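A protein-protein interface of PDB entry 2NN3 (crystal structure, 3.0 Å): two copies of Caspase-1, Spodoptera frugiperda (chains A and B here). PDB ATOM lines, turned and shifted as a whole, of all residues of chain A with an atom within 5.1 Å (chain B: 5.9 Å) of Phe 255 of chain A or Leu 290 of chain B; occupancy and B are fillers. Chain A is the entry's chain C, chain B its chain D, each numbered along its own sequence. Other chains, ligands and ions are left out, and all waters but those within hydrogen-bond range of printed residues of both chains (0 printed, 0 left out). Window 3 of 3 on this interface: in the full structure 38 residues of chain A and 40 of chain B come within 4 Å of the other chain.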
ATOM      1  N   GLU A 239     -25.035 -13.201 -14.058  1.00  0.00           N
ATOM      2  CA  GLU A 239     -24.163 -12.765 -12.984  1.00  0.00           C
ATOM      3  C   GLU A 239     -24.936 -12.574 -11.694  1.00  0.00           C
ATOM      4  O   GLU A 239     -24.609 -13.206 -10.692  1.00  0.00           O
ATOM      5  CB  GLU A 239     -23.383 -11.516 -13.363  1.00  0.00           C
ATOM      6  CG  GLU A 239     -22.223 -11.784 -14.316  1.00  0.00           C
ATOM      7  CD  GLU A 239     -21.203 -12.809 -13.777  1.00  0.00           C
ATOM      8  OE1 GLU A 239     -20.647 -12.603 -12.666  1.00  0.00           O
ATOM      9  OE2 GLU A 239     -20.947 -13.825 -14.479  1.00  0.00           O
ATOM     10  N   ARG A 247     -20.590 -11.938  -4.006  1.00  0.00           N
ATOM     11  CA  ARG A 247     -19.795 -10.843  -4.582  1.00  0.00           C
ATOM     12  C   ARG A 247     -20.402  -9.432  -4.418  1.00  0.00           C
ATOM     13  O   ARG A 247     -21.621  -9.266  -4.364  1.00  0.00           O
ATOM     14  CB  ARG A 247     -19.535 -11.111  -6.058  1.00  0.00           C
ATOM     15  CG  ARG A 247     -18.811 -12.384  -6.347  1.00  0.00           C
ATOM     16  CD  ARG A 247     -18.170 -12.283  -7.703  1.00  0.00           C
ATOM     17  NE  ARG A 247     -18.976 -12.875  -8.770  1.00  0.00           N
ATOM     18  CZ  ARG A 247     -18.639 -13.985  -9.436  1.00  0.00           C
ATOM     19  NH1 ARG A 247     -17.502 -14.627  -9.152  1.00  0.00           N
ATOM     20  NH2 ARG A 247     -19.432 -14.452 -10.402  1.00  0.00           N
ATOM     21  N   THR A 251     -17.638  -5.709  -8.682  1.00  0.00           N
ATOM     22  CA  THR A 251     -17.015  -6.894  -9.250  1.00  0.00           C
ATOM     23  C   THR A 251     -17.948  -7.590 -10.232  1.00  0.00           C
ATOM     24  O   THR A 251     -17.534  -7.968 -11.333  1.00  0.00           O
ATOM     25  CB  THR A 251     -16.646  -7.879  -8.167  1.00  0.00           C
ATOM     26  OG1 THR A 251     -15.578  -7.318  -7.403  1.00  0.00           O
ATOM     27  CG2 THR A 251     -16.216  -9.193  -8.773  1.00  0.00           C
ATOM     28  N   LEU A 252     -19.196  -7.778  -9.815  1.00  0.00           N
ATOM     29  CA  LEU A 252     -20.191  -8.395 -10.659  1.00  0.00           C
ATOM     30  C   LEU A 252     -20.253  -7.676 -12.004  1.00  0.00           C
ATOM     31  O   LEU A 252     -20.157  -8.300 -13.089  1.00  0.00           O
ATOM     32  CB  LEU A 252     -21.542  -8.259  -9.995  1.00  0.00           C
ATOM     33  CG  LEU A 252     -22.329  -9.466  -9.559  1.00  0.00           C
ATOM     34  CD1 LEU A 252     -21.715 -10.210  -8.396  1.00  0.00           C
ATOM     35  CD2 LEU A 252     -23.658  -8.926  -9.175  1.00  0.00           C
ATOM     36  N   LEU A 253     -20.408  -6.349 -11.930  1.00  0.00           N
ATOM     37  CA  LEU A 253     -20.660  -5.584 -13.104  1.00  0.00           C
ATOM     38  C   LEU A 253     -19.392  -5.597 -13.920  1.00  0.00           C
ATOM     39  O   LEU A 253     -19.442  -5.563 -15.140  1.00  0.00           O
ATOM     40  CB  LEU A 253     -21.100  -4.190 -12.727  1.00  0.00           C
ATOM     41  CG  LEU A 253     -22.558  -4.070 -12.281  1.00  0.00           C
ATOM     42  CD1 LEU A 253     -22.846  -2.661 -11.860  1.00  0.00           C
ATOM     43  CD2 LEU A 253     -23.490  -4.448 -13.396  1.00  0.00           C
ATOM     44  N   THR A 254     -18.243  -5.714 -13.267  1.00  0.00           N
ATOM     45  CA  THR A 254     -17.030  -5.876 -14.040  1.00  0.00           C
ATOM     46  C   THR A 254     -17.185  -7.050 -14.962  1.00  0.00           C
ATOM     47  O   THR A 254     -16.924  -6.944 -16.145  1.00  0.00           O
ATOM     48  CB  THR A 254     -15.786  -6.073 -13.189  1.00  0.00           C
ATOM     49  OG1 THR A 254     -15.510  -4.853 -12.501  1.00  0.00           O
ATOM     50  CG2 THR A 254     -14.608  -6.411 -14.083  1.00  0.00           C
ATOM     51  N   PHE A 255     -17.643  -8.164 -14.406  1.00  0.00           N
ATOM     52  CA  PHE A 255     -17.714  -9.405 -15.144  1.00  0.00           C
ATOM     53  C   PHE A 255     -18.759  -9.329 -16.231  1.00  0.00           C
ATOM     54  O   PHE A 255     -18.538  -9.847 -17.304  1.00  0.00           O
ATOM     55  CB  PHE A 255     -17.939 -10.589 -14.208  1.00  0.00           C
ATOM     56  CG  PHE A 255     -16.774 -10.863 -13.282  1.00  0.00           C
ATOM     57  CD1 PHE A 255     -16.984 -11.403 -12.021  1.00  0.00           C
ATOM     58  CD2 PHE A 255     -15.458 -10.571 -13.679  1.00  0.00           C
ATOM     59  CE1 PHE A 255     -15.902 -11.652 -11.163  1.00  0.00           C
ATOM     60  CE2 PHE A 255     -14.354 -10.810 -12.830  1.00  0.00           C
ATOM     61  CZ  PHE A 255     -14.577 -11.349 -11.566  1.00  0.00           C
ATOM     62  N   VAL A 256     -19.864  -8.632 -15.980  1.00  0.00           N
ATOM     63  CA  VAL A 256     -20.817  -8.369 -17.052  1.00  0.00           C
ATOM     64  C   VAL A 256     -20.109  -7.704 -18.236  1.00  0.00           C
ATOM     65  O   VAL A 256     -20.257  -8.134 -19.372  1.00  0.00           O
ATOM     66  CB  VAL A 256     -22.011  -7.503 -16.589  1.00  0.00           C
ATOM     67  CG1 VAL A 256     -22.990  -7.241 -17.767  1.00  0.00           C
ATOM     68  CG2 VAL A 256     -22.728  -8.148 -15.404  1.00  0.00           C
ATOM     69  N   CYS A 257     -19.323  -6.667 -17.974  1.00  0.00           N
ATOM     70  CA  CYS A 257     -18.573  -6.031 -19.049  1.00  0.00           C
ATOM     71  C   CYS A 257     -17.816  -7.054 -19.849  1.00  0.00           C
ATOM     72  O   CYS A 257     -18.020  -7.137 -21.070  1.00  0.00           O
ATOM     73  CB  CYS A 257     -17.658  -4.936 -18.532  1.00  0.00           C
ATOM     74  SG  CYS A 257     -18.695  -3.562 -18.005  1.00  0.00           S
ATOM     75  N   GLN A 258     -17.009  -7.870 -19.157  1.00  0.00           N
ATOM     76  CA  GLN A 258     -16.206  -8.905 -19.793  1.00  0.00           C
ATOM     77  C   GLN A 258     -17.032  -9.768 -20.724  1.00  0.00           C
ATOM     78  O   GLN A 258     -16.662  -9.998 -21.868  1.00  0.00           O
ATOM     79  CB  GLN A 258     -15.540  -9.776 -18.754  1.00  0.00           C
ATOM     80  CG  GLN A 258     -14.625 -10.790 -19.378  1.00  0.00           C
ATOM     81  CD  GLN A 258     -13.501 -11.204 -18.482  1.00  0.00           C
ATOM     82  OE1 GLN A 258     -13.623 -11.160 -17.259  1.00  0.00           O
ATOM     83  NE2 GLN A 258     -12.380 -11.621 -19.085  1.00  0.00           N
ATOM     84  N   LYS A 259     -18.169 -10.223 -20.234  1.00  0.00           N
ATOM     85  CA  LYS A 259     -19.058 -11.015 -21.049  1.00  0.00           C
ATOM     86  C   LYS A 259     -19.448 -10.236 -22.317  1.00  0.00           C
ATOM     87  O   LYS A 259     -19.303 -10.787 -23.421  1.00  0.00           O
ATOM     88  CB  LYS A 259     -20.292 -11.511 -20.252  1.00  0.00           C
ATOM     89  N   PRO B  51      -9.801 -13.676 -14.776  1.00  0.00           N
ATOM     90  CA  PRO B  51     -10.447 -12.719 -13.879  1.00  0.00           C
ATOM     91  C   PRO B  51      -9.649 -11.435 -13.622  1.00  0.00           C
ATOM     92  O   PRO B  51     -10.223 -10.422 -13.227  1.00  0.00           O
ATOM     93  CB  PRO B  51     -10.574 -13.509 -12.569  1.00  0.00           C
ATOM     94  CG  PRO B  51     -10.262 -14.929 -12.922  1.00  0.00           C
ATOM     95  CD  PRO B  51      -9.301 -14.841 -14.035  1.00  0.00           C
ATOM     96  N   TYR B  52      -8.342 -11.490 -13.841  1.00  0.00           N
ATOM     97  CA  TYR B  52      -7.450 -10.429 -13.427  1.00  0.00           C
ATOM     98  C   TYR B  52      -6.593  -9.939 -14.559  1.00  0.00           C
ATOM     99  O   TYR B  52      -6.337 -10.664 -15.513  1.00  0.00           O
ATOM    100  CB  TYR B  52      -6.526 -10.935 -12.332  1.00  0.00           C
ATOM    101  CG  TYR B  52      -7.164 -11.085 -10.982  1.00  0.00           C
ATOM    102  CD1 TYR B  52      -7.365 -12.332 -10.435  1.00  0.00           C
ATOM    103  CD2 TYR B  52      -7.551  -9.977 -10.249  1.00  0.00           C
ATOM    104  CE1 TYR B  52      -7.943 -12.470  -9.186  1.00  0.00           C
ATOM    105  CE2 TYR B  52      -8.133 -10.103  -9.010  1.00  0.00           C
ATOM    106  CZ  TYR B  52      -8.323 -11.347  -8.477  1.00  0.00           C
ATOM    107  OH  TYR B  52      -8.890 -11.484  -7.228  1.00  0.00           O
ATOM    108  N   TYR B  53      -6.127  -8.702 -14.431  1.00  0.00           N
ATOM    109  CA  TYR B  53      -5.201  -8.165 -15.390  1.00  0.00           C
ATOM    110  C   TYR B  53      -3.842  -8.719 -15.108  1.00  0.00           C
ATOM    111  O   TYR B  53      -3.436  -8.815 -13.947  1.00  0.00           O
ATOM    112  CB  TYR B  53      -5.138  -6.656 -15.292  1.00  0.00           C
ATOM    113  CG  TYR B  53      -6.287  -5.965 -15.961  1.00  0.00           C
ATOM    114  CD1 TYR B  53      -6.346  -5.858 -17.337  1.00  0.00           C
ATOM    115  CD2 TYR B  53      -7.312  -5.415 -15.211  1.00  0.00           C
ATOM    116  CE1 TYR B  53      -7.394  -5.241 -17.946  1.00  0.00           C
ATOM    117  CE2 TYR B  53      -8.364  -4.780 -15.812  1.00  0.00           C
ATOM    118  CZ  TYR B  53      -8.404  -4.699 -17.181  1.00  0.00           C
ATOM    119  OH  TYR B  53      -9.467  -4.058 -17.780  1.00  0.00           O
ATOM    120  N   ASP B 248      -8.529  -4.739  -5.028  1.00  0.00           N
ATOM    121  CA  ASP B 248      -8.786  -4.311  -6.401  1.00  0.00           C
ATOM    122  C   ASP B 248      -9.019  -2.814  -6.497  1.00  0.00           C
ATOM    123  O   ASP B 248      -9.524  -2.197  -5.566  1.00  0.00           O
ATOM    124  CB  ASP B 248      -9.986  -5.078  -6.987  1.00  0.00           C
ATOM    125  CG  ASP B 248     -11.356  -4.454  -6.610  1.00  0.00           C
ATOM    126  OD1 ASP B 248     -12.273  -4.420  -7.484  1.00  0.00           O
ATOM    127  OD2 ASP B 248     -11.523  -3.994  -5.449  1.00  0.00           O
ATOM    128  N   LEU B 287     -13.664  -1.160 -17.205  1.00  0.00           N
ATOM    129  CA  LEU B 287     -12.747  -2.287 -16.972  1.00  0.00           C
ATOM    130  C   LEU B 287     -13.424  -3.652 -17.200  1.00  0.00           C
ATOM    131  O   LEU B 287     -14.614  -3.828 -16.866  1.00  0.00           O
ATOM    132  CB  LEU B 287     -12.187  -2.239 -15.557  1.00  0.00           C
ATOM    133  CG  LEU B 287     -11.405  -1.004 -15.165  1.00  0.00           C
ATOM    134  CD1 LEU B 287     -10.683  -1.280 -13.887  1.00  0.00           C
ATOM    135  CD2 LEU B 287     -10.397  -0.598 -16.244  1.00  0.00           C
ATOM    136  N   THR B 288     -12.652  -4.607 -17.742  1.00  0.00           N
ATOM    137  CA  THR B 288     -13.132  -5.979 -18.022  1.00  0.00           C
ATOM    138  C   THR B 288     -12.568  -7.083 -17.113  1.00  0.00           C
ATOM    139  O   THR B 288     -12.956  -8.254 -17.254  1.00  0.00           O
ATOM    140  CB  THR B 288     -12.793  -6.401 -19.444  1.00  0.00           C
ATOM    141  OG1 THR B 288     -11.418  -6.099 -19.698  1.00  0.00           O
ATOM    142  CG2 THR B 288     -13.685  -5.693 -20.443  1.00  0.00           C
ATOM    143  N   ARG B 289     -11.630  -6.729 -16.224  1.00  0.00           N
ATOM    144  CA  ARG B 289     -11.073  -7.678 -15.260  1.00  0.00           C
ATOM    145  C   ARG B 289     -10.910  -6.938 -13.978  1.00  0.00           C
ATOM    146  O   ARG B 289     -10.862  -5.719 -14.001  1.00  0.00           O
ATOM    147  CB  ARG B 289      -9.697  -8.193 -15.686  1.00  0.00           C
ATOM    148  CG  ARG B 289      -9.494  -8.332 -17.163  1.00  0.00           C
ATOM    149  CD  ARG B 289      -8.744  -9.579 -17.577  1.00  0.00           C
ATOM    150  NE  ARG B 289      -9.197  -9.905 -18.924  1.00  0.00           N
ATOM    151  CZ  ARG B 289      -9.042 -11.072 -19.533  1.00  0.00           C
ATOM    152  NH1 ARG B 289      -8.410 -12.065 -18.927  1.00  0.00           N
ATOM    153  NH2 ARG B 289      -9.525 -11.246 -20.760  1.00  0.00           N
ATOM    154  N   LEU B 290     -10.819  -7.652 -12.860  1.00  0.00           N
ATOM    155  CA  LEU B 290     -10.387  -7.041 -11.617  1.00  0.00           C
ATOM    156  C   LEU B 290      -8.949  -6.563 -11.829  1.00  0.00           C
ATOM    157  O   LEU B 290      -8.167  -7.230 -12.514  1.00  0.00           O
ATOM    158  CB  LEU B 290     -10.403  -8.044 -10.461  1.00  0.00           C
ATOM    159  CG  LEU B 290     -11.566  -8.552  -9.585  1.00  0.00           C
ATOM    160  CD1 LEU B 290     -12.603  -7.487  -9.291  1.00  0.00           C
ATOM    161  CD2 LEU B 290     -12.213  -9.768 -10.192  1.00  0.00           C
ATOM    162  N   LEU B 291      -8.605  -5.414 -11.254  1.00  0.00           N
ATOM    163  CA  LEU B 291      -7.261  -4.863 -11.384  1.00  0.00           C
ATOM    164  C   LEU B 291      -6.566  -4.757 -10.036  1.00  0.00           C
ATOM    165  O   LEU B 291      -6.776  -3.800  -9.287  1.00  0.00           O
ATOM    166  CB  LEU B 291      -7.314  -3.491 -12.047  1.00  0.00           C
ATOM    167  CG  LEU B 291      -5.983  -2.753 -12.229  1.00  0.00           C
ATOM    168  CD1 LEU B 291      -5.151  -3.427 -13.313  1.00  0.00           C
ATOM    169  CD2 LEU B 291      -6.194  -1.278 -12.562  1.00  0.00           C
ATOM    170  N   VAL B 292      -5.735  -5.741  -9.723  1.00  0.00           N
ATOM    171  CA  VAL B 292      -4.964  -5.695  -8.488  1.00  0.00           C
ATOM    172  C   VAL B 292      -3.548  -5.278  -8.819  1.00  0.00           C
ATOM    173  O   VAL B 292      -2.923  -5.876  -9.705  1.00  0.00           O
ATOM    174  CB  VAL B 292      -4.929  -7.058  -7.793  1.00  0.00           C
ATOM    175  CG1 VAL B 292      -4.211  -6.954  -6.437  1.00  0.00           C
ATOM    176  CG2 VAL B 292      -6.336  -7.582  -7.606  1.00  0.00           C
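Printed residues of chain B within 4 Å of Thr 251 of chain A: Leu 290 (3.5 Å).
Leu 252 of chain A touches none of the printed residues of chain B.
Phe 255 of chain A touches just one residue of chain B: Leu 290 (3.2 Å).
Of the printed residues of chain B, Cys 257 of chain A touches Leu 287 (3.6 Å).
Of the printed residues of chain B, Gln 258 of chain A touches Thr 288 and Arg 289.
Of the 10 printed residues of chain B, 4 touch a printed residue of chain A.
Printed residues of chain B that touch a printed residue of chain A: Leu 287, Thr 288, Arg 289 and Leu 290.
Hydrophobic or aromatic side chains of chain B that line the printed part of chain A: Leu 290.
Among the printed residues, no Asp or Glu carboxylate lies within 4 Å of a Lys or Arg side-chain nitrogen of the other chain.
The side-chain sulfur of Cys 257 of chain A is in hydrogen-bond range of the backbone carbonyl oxygen of Leu 253 of chain A, 3.6 Å away.
The backbone carbonyl oxygen (O) of Pro 51 of chain B sits at hydrogen-bond distance from the backbone NH (N) of Leu 290 of chain B.
The backbone NH of Thr 288 of chain B sits at hydrogen-bond distance from the side-chain hydroxyl of Tyr 53 of chain B.
O of Leu 290 of chain B sits at hydrogen-bond distance from N of Tyr 53 of chain B, at 3.2 Å.
No position is printed for both chains.
The side-chain amide nitrogen of Gln 258 of chain A lies close to the guanidinium group of Arg 289 of chain B (3.3 Å).
OE1 of Gln 258 of chain A sits close to O of Thr 288 of chain B.
Among the printed residues, pairs that only touch across the chains: Phe 255 of chain A with Leu 290 of chain B, Thr 251 of chain A with Leu 290 of chain B, Cys 257 of chain A with Leu 287 of chain B, Thr 254 of chain A with Arg 289 of chain B, Thr 254 of chain A with Thr 288 of chain B and Thr 254 of chain A with Leu 287 of chain B.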
